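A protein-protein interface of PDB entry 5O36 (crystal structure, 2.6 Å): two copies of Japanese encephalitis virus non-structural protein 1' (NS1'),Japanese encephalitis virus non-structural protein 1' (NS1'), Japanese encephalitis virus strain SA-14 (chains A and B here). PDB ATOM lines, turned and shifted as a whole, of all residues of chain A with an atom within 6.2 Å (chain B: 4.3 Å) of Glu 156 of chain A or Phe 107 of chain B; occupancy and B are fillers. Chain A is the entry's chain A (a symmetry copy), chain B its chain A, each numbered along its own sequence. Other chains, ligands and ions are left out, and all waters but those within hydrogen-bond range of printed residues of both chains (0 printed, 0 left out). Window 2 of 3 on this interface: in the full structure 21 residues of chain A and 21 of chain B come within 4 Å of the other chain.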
ATOM      1  N   GLU A 100     -30.768  13.285  32.838  1.00  0.00           N
ATOM      2  CA  GLU A 100     -29.701  13.078  31.859  1.00  0.00           C
ATOM      3  C   GLU A 100     -28.658  12.144  32.491  1.00  0.00           C
ATOM      4  O   GLU A 100     -28.890  11.551  33.531  1.00  0.00           O
ATOM      5  CB  GLU A 100     -29.131  14.433  31.398  1.00  0.00           C
ATOM      6  CG  GLU A 100     -30.193  15.488  30.998  1.00  0.00           C
ATOM      7  CD  GLU A 100     -30.625  15.456  29.521  1.00  0.00           C
ATOM      8  OE1 GLU A 100     -31.296  16.425  29.055  1.00  0.00           O
ATOM      9  OE2 GLU A 100     -30.285  14.478  28.817  1.00  0.00           O
ATOM     10  N   ASN A 101     -27.533  11.963  31.832  1.00  0.00           N
ATOM     11  CA  ASN A 101     -26.437  11.125  32.362  1.00  0.00           C
ATOM     12  C   ASN A 101     -25.097  11.856  32.079  1.00  0.00           C
ATOM     13  O   ASN A 101     -25.001  12.655  31.139  1.00  0.00           O
ATOM     14  CB  ASN A 101     -26.512   9.741  31.699  1.00  0.00           C
ATOM     15  CG  ASN A 101     -25.958   8.623  32.569  1.00  0.00           C
ATOM     16  OD1 ASN A 101     -26.659   8.065  33.433  1.00  0.00           O
ATOM     17  ND2 ASN A 101     -24.697   8.266  32.320  1.00  0.00           N
ATOM     18  N   GLY A 102     -24.095  11.659  32.925  1.00  0.00           N
ATOM     19  CA  GLY A 102     -22.873  12.517  32.879  1.00  0.00           C
ATOM     20  C   GLY A 102     -22.973  14.032  33.218  1.00  0.00           C
ATOM     21  O   GLY A 102     -22.208  14.839  32.694  1.00  0.00           O
ATOM     22  N   ARG A 154     -24.533  21.266  33.519  1.00  0.00           N
ATOM     23  CA  ARG A 154     -24.210  20.869  32.129  1.00  0.00           C
ATOM     24  C   ARG A 154     -24.530  19.431  31.908  1.00  0.00           C
ATOM     25  O   ARG A 154     -24.124  18.585  32.711  1.00  0.00           O
ATOM     26  CB  ARG A 154     -22.775  21.116  31.784  1.00  0.00           C
ATOM     27  CG  ARG A 154     -22.466  22.595  31.824  1.00  0.00           C
ATOM     28  CD  ARG A 154     -20.998  22.835  31.575  1.00  0.00           C
ATOM     29  NE  ARG A 154     -20.184  22.449  32.732  1.00  0.00           N
ATOM     30  CZ  ARG A 154     -18.855  22.330  32.710  1.00  0.00           C
ATOM     31  NH1 ARG A 154     -18.163  22.540  31.584  1.00  0.00           N
ATOM     32  NH2 ARG A 154     -18.209  21.990  33.822  1.00  0.00           N
ATOM     33  N   THR A 155     -25.304  19.188  30.835  1.00  0.00           N
ATOM     34  CA  THR A 155     -25.624  17.862  30.350  1.00  0.00           C
ATOM     35  C   THR A 155     -25.050  17.659  28.964  1.00  0.00           C
ATOM     36  O   THR A 155     -24.454  18.563  28.410  1.00  0.00           O
ATOM     37  CB  THR A 155     -27.115  17.695  30.285  1.00  0.00           C
ATOM     38  OG1 THR A 155     -27.678  18.605  29.324  1.00  0.00           O
ATOM     39  CG2 THR A 155     -27.706  17.906  31.645  1.00  0.00           C
ATOM     40  N   GLU A 156     -25.188  16.467  28.391  1.00  0.00           N
ATOM     41  CA  GLU A 156     -24.595  16.222  27.055  1.00  0.00           C
ATOM     42  C   GLU A 156     -25.056  17.280  26.054  1.00  0.00           C
ATOM     43  O   GLU A 156     -24.296  17.754  25.227  1.00  0.00           O
ATOM     44  CB  GLU A 156     -24.936  14.824  26.513  1.00  0.00           C
ATOM     45  CG  GLU A 156     -23.786  14.268  25.691  1.00  0.00           C
ATOM     46  CD  GLU A 156     -24.153  13.133  24.749  1.00  0.00           C
ATOM     47  OE1 GLU A 156     -25.247  12.543  24.902  1.00  0.00           O
ATOM     48  OE2 GLU A 156     -23.315  12.833  23.863  1.00  0.00           O
ATOM     49  N   ASN A 157     -26.317  17.641  26.182  1.00  0.00           N
ATOM     50  CA  ASN A 157     -27.041  18.270  25.135  1.00  0.00           C
ATOM     51  C   ASN A 157     -27.125  19.776  25.372  1.00  0.00           C
ATOM     52  O   ASN A 157     -27.184  20.512  24.408  1.00  0.00           O
ATOM     53  CB  ASN A 157     -28.431  17.570  24.923  1.00  0.00           C
ATOM     54  CG  ASN A 157     -29.311  17.498  26.212  1.00  0.00           C
ATOM     55  OD1 ASN A 157     -29.114  16.625  27.090  1.00  0.00           O
ATOM     56  ND2 ASN A 157     -30.311  18.391  26.293  1.00  0.00           N
ATOM     57  N   GLY A 158     -27.106  20.245  26.621  1.00  0.00           N
ATOM     58  CA  GLY A 158     -27.020  21.688  26.892  1.00  0.00           C
ATOM     59  C   GLY A 158     -26.569  22.187  28.262  1.00  0.00           C
ATOM     60  O   GLY A 158     -26.163  21.414  29.137  1.00  0.00           O
ATOM     61  N   LEU B  42     -16.109   3.053  23.759  1.00  0.00           N
ATOM     62  CA  LEU B  42     -16.220   4.057  24.758  1.00  0.00           C
ATOM     63  C   LEU B  42     -17.338   5.113  24.419  1.00  0.00           C
ATOM     64  O   LEU B  42     -17.385   5.726  23.352  1.00  0.00           O
ATOM     65  CB  LEU B  42     -14.843   4.696  24.972  1.00  0.00           C
ATOM     66  CG  LEU B  42     -14.786   5.732  26.092  1.00  0.00           C
ATOM     67  CD1 LEU B  42     -15.013   5.113  27.485  1.00  0.00           C
ATOM     68  CD2 LEU B  42     -13.470   6.516  26.028  1.00  0.00           C
ATOM     69  N   GLU B  43     -18.240   5.296  25.362  1.00  0.00           N
ATOM     70  CA  GLU B  43     -19.332   6.189  25.206  1.00  0.00           C
ATOM     71  C   GLU B  43     -19.025   7.513  25.869  1.00  0.00           C
ATOM     72  O   GLU B  43     -19.067   8.565  25.237  1.00  0.00           O
ATOM     73  CB  GLU B  43     -20.592   5.578  25.811  1.00  0.00           C
ATOM     74  CG  GLU B  43     -21.815   6.244  25.225  1.00  0.00           C
ATOM     75  CD  GLU B  43     -23.109   5.881  25.901  1.00  0.00           C
ATOM     76  OE1 GLU B  43     -23.164   4.935  26.729  1.00  0.00           O
ATOM     77  OE2 GLU B  43     -24.086   6.560  25.565  1.00  0.00           O
ATOM     78  N   ARG B  44     -18.775   7.466  27.170  1.00  0.00           N
ATOM     79  CA  ARG B  44     -18.516   8.680  27.931  1.00  0.00           C
ATOM     80  C   ARG B  44     -17.743   8.361  29.196  1.00  0.00           C
ATOM     81  O   ARG B  44     -17.770   7.231  29.679  1.00  0.00           O
ATOM     82  CB  ARG B  44     -19.811   9.454  28.243  1.00  0.00           C
ATOM     83  CG  ARG B  44     -20.503   9.007  29.489  1.00  0.00           C
ATOM     84  CD  ARG B  44     -21.759   9.810  29.756  1.00  0.00           C
ATOM     85  NE  ARG B  44     -22.924   9.040  29.347  1.00  0.00           N
ATOM     86  CZ  ARG B  44     -23.629   9.228  28.233  1.00  0.00           C
ATOM     87  NH1 ARG B  44     -23.347  10.199  27.347  1.00  0.00           N
ATOM     88  NH2 ARG B  44     -24.644   8.409  27.986  1.00  0.00           N
ATOM     89  N   ARG B  87     -12.151   3.941  20.870  1.00  0.00           N
ATOM     90  CA  ARG B  87     -13.075   4.445  19.851  1.00  0.00           C
ATOM     91  C   ARG B  87     -12.316   4.350  18.549  1.00  0.00           C
ATOM     92  O   ARG B  87     -11.121   4.615  18.486  1.00  0.00           O
ATOM     93  CB  ARG B  87     -13.533   5.888  20.155  1.00  0.00           C
ATOM     94  CG  ARG B  87     -14.749   6.397  19.387  1.00  0.00           C
ATOM     95  CD  ARG B  87     -16.090   6.144  20.060  1.00  0.00           C
ATOM     96  NE  ARG B  87     -17.254   6.679  19.325  1.00  0.00           N
ATOM     97  CZ  ARG B  87     -18.489   6.839  19.831  1.00  0.00           C
ATOM     98  NH1 ARG B  87     -18.781   6.498  21.088  1.00  0.00           N
ATOM     99  NH2 ARG B  87     -19.448   7.375  19.089  1.00  0.00           N
ATOM    100  N   LEU B 105     -15.861  13.513  29.137  1.00  0.00           N
ATOM    101  CA  LEU B 105     -15.407  13.073  27.824  1.00  0.00           C
ATOM    102  C   LEU B 105     -16.535  12.320  27.164  1.00  0.00           C
ATOM    103  O   LEU B 105     -17.023  11.354  27.705  1.00  0.00           O
ATOM    104  CB  LEU B 105     -14.211  12.141  27.993  1.00  0.00           C
ATOM    105  CG  LEU B 105     -13.327  11.838  26.779  1.00  0.00           C
ATOM    106  CD1 LEU B 105     -12.175  10.944  27.192  1.00  0.00           C
ATOM    107  CD2 LEU B 105     -14.082  11.147  25.687  1.00  0.00           C
ATOM    108  N   ASP B 106     -16.944  12.746  25.988  1.00  0.00           N
ATOM    109  CA  ASP B 106     -17.930  12.020  25.218  1.00  0.00           C
ATOM    110  C   ASP B 106     -17.720  12.246  23.705  1.00  0.00           C
ATOM    111  O   ASP B 106     -16.625  12.688  23.269  1.00  0.00           O
ATOM    112  CB  ASP B 106     -19.304  12.420  25.667  1.00  0.00           C
ATOM    113  CG  ASP B 106     -19.519  13.897  25.576  1.00  0.00           C
ATOM    114  OD1 ASP B 106     -18.785  14.608  24.839  1.00  0.00           O
ATOM    115  OD2 ASP B 106     -20.429  14.354  26.286  1.00  0.00           O
ATOM    116  N   PHE B 107     -18.717  11.857  22.902  1.00  0.00           N
ATOM    117  CA  PHE B 107     -18.601  11.931  21.472  1.00  0.00           C
ATOM    118  C   PHE B 107     -19.818  12.637  20.918  1.00  0.00           C
ATOM    119  O   PHE B 107     -20.929  12.086  20.800  1.00  0.00           O
ATOM    120  CB  PHE B 107     -18.398  10.555  20.884  1.00  0.00           C
ATOM    121  CG  PHE B 107     -17.171   9.882  21.370  1.00  0.00           C
ATOM    122  CD1 PHE B 107     -17.183   9.175  22.562  1.00  0.00           C
ATOM    123  CD2 PHE B 107     -15.982   9.977  20.667  1.00  0.00           C
ATOM    124  CE1 PHE B 107     -16.011   8.545  23.032  1.00  0.00           C
ATOM    125  CE2 PHE B 107     -14.809   9.339  21.136  1.00  0.00           C
ATOM    126  CZ  PHE B 107     -14.822   8.625  22.309  1.00  0.00           C
ATOM    127  N   ASP B 108     -19.572  13.904  20.616  1.00  0.00           N
ATOM    128  CA  ASP B 108     -20.603  14.850  20.283  1.00  0.00           C
ATOM    129  C   ASP B 108     -19.924  16.151  19.776  1.00  0.00           C
ATOM    130  O   ASP B 108     -18.728  16.381  19.989  1.00  0.00           O
ATOM    131  CB  ASP B 108     -21.478  15.089  21.532  1.00  0.00           C
ATOM    132  CG  ASP B 108     -22.831  15.700  21.204  1.00  0.00           C
ATOM    133  OD1 ASP B 108     -23.170  15.704  19.988  1.00  0.00           O
ATOM    134  OD2 ASP B 108     -23.545  16.183  22.141  1.00  0.00           O
ATOM    135  N   PRO B 149     -19.624  10.752  15.576  1.00  0.00           N
ATOM    136  CA  PRO B 149     -19.386  12.107  16.172  1.00  0.00           C
ATOM    137  C   PRO B 149     -18.039  12.247  16.888  1.00  0.00           C
ATOM    138  O   PRO B 149     -17.517  11.257  17.346  1.00  0.00           O
ATOM    139  CB  PRO B 149     -20.520  12.250  17.210  1.00  0.00           C
ATOM    140  CG  PRO B 149     -21.161  10.929  17.348  1.00  0.00           C
ATOM    141  CD  PRO B 149     -20.589   9.965  16.357  1.00  0.00           C
ATOM    142  N   PRO B 150     -17.497  13.479  16.991  1.00  0.00           N
ATOM    143  CA  PRO B 150     -16.111  13.684  17.411  1.00  0.00           C
ATOM    144  C   PRO B 150     -15.888  13.555  18.922  1.00  0.00           C
ATOM    145  O   PRO B 150     -16.820  13.800  19.740  1.00  0.00           O
ATOM    146  CB  PRO B 150     -15.839  15.113  16.979  1.00  0.00           C
ATOM    147  CG  PRO B 150     -17.165  15.795  17.147  1.00  0.00           C
ATOM    148  CD  PRO B 150     -18.187  14.764  16.778  1.00  0.00           C
ATOM    149  N   LEU B 151     -14.647  13.183  19.257  1.00  0.00           N
ATOM    150  CA  LEU B 151     -14.183  13.129  20.624  1.00  0.00           C
ATOM    151  C   LEU B 151     -14.197  14.518  21.265  1.00  0.00           C
ATOM    152  O   LEU B 151     -13.467  15.394  20.855  1.00  0.00           O
ATOM    153  CB  LEU B 151     -12.787  12.528  20.694  1.00  0.00           C
ATOM    154  CG  LEU B 151     -12.382  11.952  22.063  1.00  0.00           C
ATOM    155  CD1 LEU B 151     -11.180  11.041  21.948  1.00  0.00           C
ATOM    156  CD2 LEU B 151     -12.077  13.034  23.081  1.00  0.00           C
ATOM    157  N   ARG B 152     -15.002  14.676  22.314  1.00  0.00           N
ATOM    158  CA  ARG B 152     -15.177  15.945  23.024  1.00  0.00           C
ATOM    159  C   ARG B 152     -14.787  15.904  24.516  1.00  0.00           C
ATOM    160  O   ARG B 152     -15.279  15.059  25.246  1.00  0.00           O
ATOM    161  CB  ARG B 152     -16.642  16.306  22.924  1.00  0.00           C
ATOM    162  CG  ARG B 152     -16.994  17.636  23.502  1.00  0.00           C
ATOM    163  CD  ARG B 152     -18.424  17.934  23.188  1.00  0.00           C
ATOM    164  NE  ARG B 152     -19.363  17.224  24.036  1.00  0.00           N
ATOM    165  CZ  ARG B 152     -20.655  17.544  24.164  1.00  0.00           C
ATOM    166  NH1 ARG B 152     -21.211  18.516  23.457  1.00  0.00           N
ATOM    167  NH2 ARG B 152     -21.420  16.854  24.982  1.00  0.00           N
ATOM    168  N   ARG B 154     -15.255  18.434  27.863  1.00  0.00           N
ATOM    169  CA  ARG B 154     -15.781  19.662  28.506  1.00  0.00           C
ATOM    170  C   ARG B 154     -15.158  19.858  29.845  1.00  0.00           C
ATOM    171  O   ARG B 154     -15.129  18.920  30.648  1.00  0.00           O
ATOM    172  CB  ARG B 154     -17.270  19.637  28.651  1.00  0.00           C
ATOM    173  CG  ARG B 154     -17.935  19.620  27.294  1.00  0.00           C
ATOM    174  CD  ARG B 154     -19.431  19.493  27.441  1.00  0.00           C
ATOM    175  NE  ARG B 154     -19.821  18.140  27.850  1.00  0.00           N
ATOM    176  CZ  ARG B 154     -21.040  17.806  28.280  1.00  0.00           C
ATOM    177  NH1 ARG B 154     -22.007  18.725  28.389  1.00  0.00           N
ATOM    178  NH2 ARG B 154     -21.295  16.543  28.611  1.00  0.00           N
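Position printed for both chains: 154.
Of the 8 pairs that touch across the chains among the printed residues, none has its exchanged pair printed and touching as well.
The side-chain carboxylate (OE1) of Glu 156 of chain A lies within salt-bridge range of the guanidinium group (NH1) of Arg 44 of chain B, 3.9 Å away.
O of Glu 156 of chain A lies within hydrogen-bond range of NH2 of Arg 152 of chain B (3.0 Å).
The guanidinium group of Arg 154 of chain B sits at hydrogen-bond distance from the backbone carbonyl oxygen of Thr 155 of chain A, at 2.5 Å.
Printed residues of chain A that touch a printed residue of chain B: Asn 101, Thr 155 and Glu 156.
Among the printed residues, 8 pairs touch across the chains.
Among the printed residues, Asp or Glu carboxylates within 4 Å of a Lys or Arg side-chain nitrogen of the other chain: Glu 156 of chain A with Arg 44 of chain B (3.9 Å).
The side-chain hydroxyl (OG1) of Thr 155 of chain A is in hydrogen-bond range of the backbone carbonyl oxygen (O) of Gly 158 of chain A, at 3.2 Å.
The guanidinium group of Arg 154 of chain B is in salt-bridge range of the side-chain carboxylate of Asp 106 of chain B (3.3 Å).
O of Pro 150 of chain B lies within hydrogen-bond range of N of Asp 108 of chain B.
The side-chain carboxylate (OD1) of Asp 106 of chain B lies within salt-bridge range of the guanidinium group (NE) of Arg 152 of chain B (2.8 Å).
NH1 of Arg 152 of chain B is in salt-bridge range of OD2 of Asp 108 of chain B (3.6 Å).
The side-chain hydroxyl (OG1) of Thr 155 of chain A sits at hydrogen-bond distance from the side-chain amide oxygen (OD1) of Asn 157 of chain A (3.3 Å).
Printed residues of chain B within 4 Å of Thr 155 of chain A: Arg 154.
Printed residues of chain A within 4 Å of Arg 44 of chain B: Asn 101 and Glu 156.
Printed residues of chain A within 4 Å of Asp 106 of chain B: Glu 156 (3.4 Å).
Phe 107 of chain B touches just one residue of chain A: Glu 156.
Printed residues of chain A within 4 Å of Arg 152 of chain B: Glu 156.
Of the printed residues of chain A, Arg 154 of chain B touches Thr 155 and Glu 156.
The nearest printed residue of chain B that does not touch Glu 156 of chain A is Glu 43 of chain B (6.1 Å).
The nearest printed residue of chain A that does not touch Phe 107 of chain B is Asn 157 of chain A (9.4 Å).
Among the printed residues, pairs that only touch across the chains: Glu 156 of chain A with Asp 106 of chain B (3.4 Å), Glu 156 of chain A with Asp 108 of chain B (3.5 Å), Asn 101 of chain A with Arg 44 of chain B (3.5 Å), Glu 156 of chain A with Arg 154 of chain B (3.7 Å) and Glu 156 of chain A with Phe 107 of chain B (3.95 Å).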
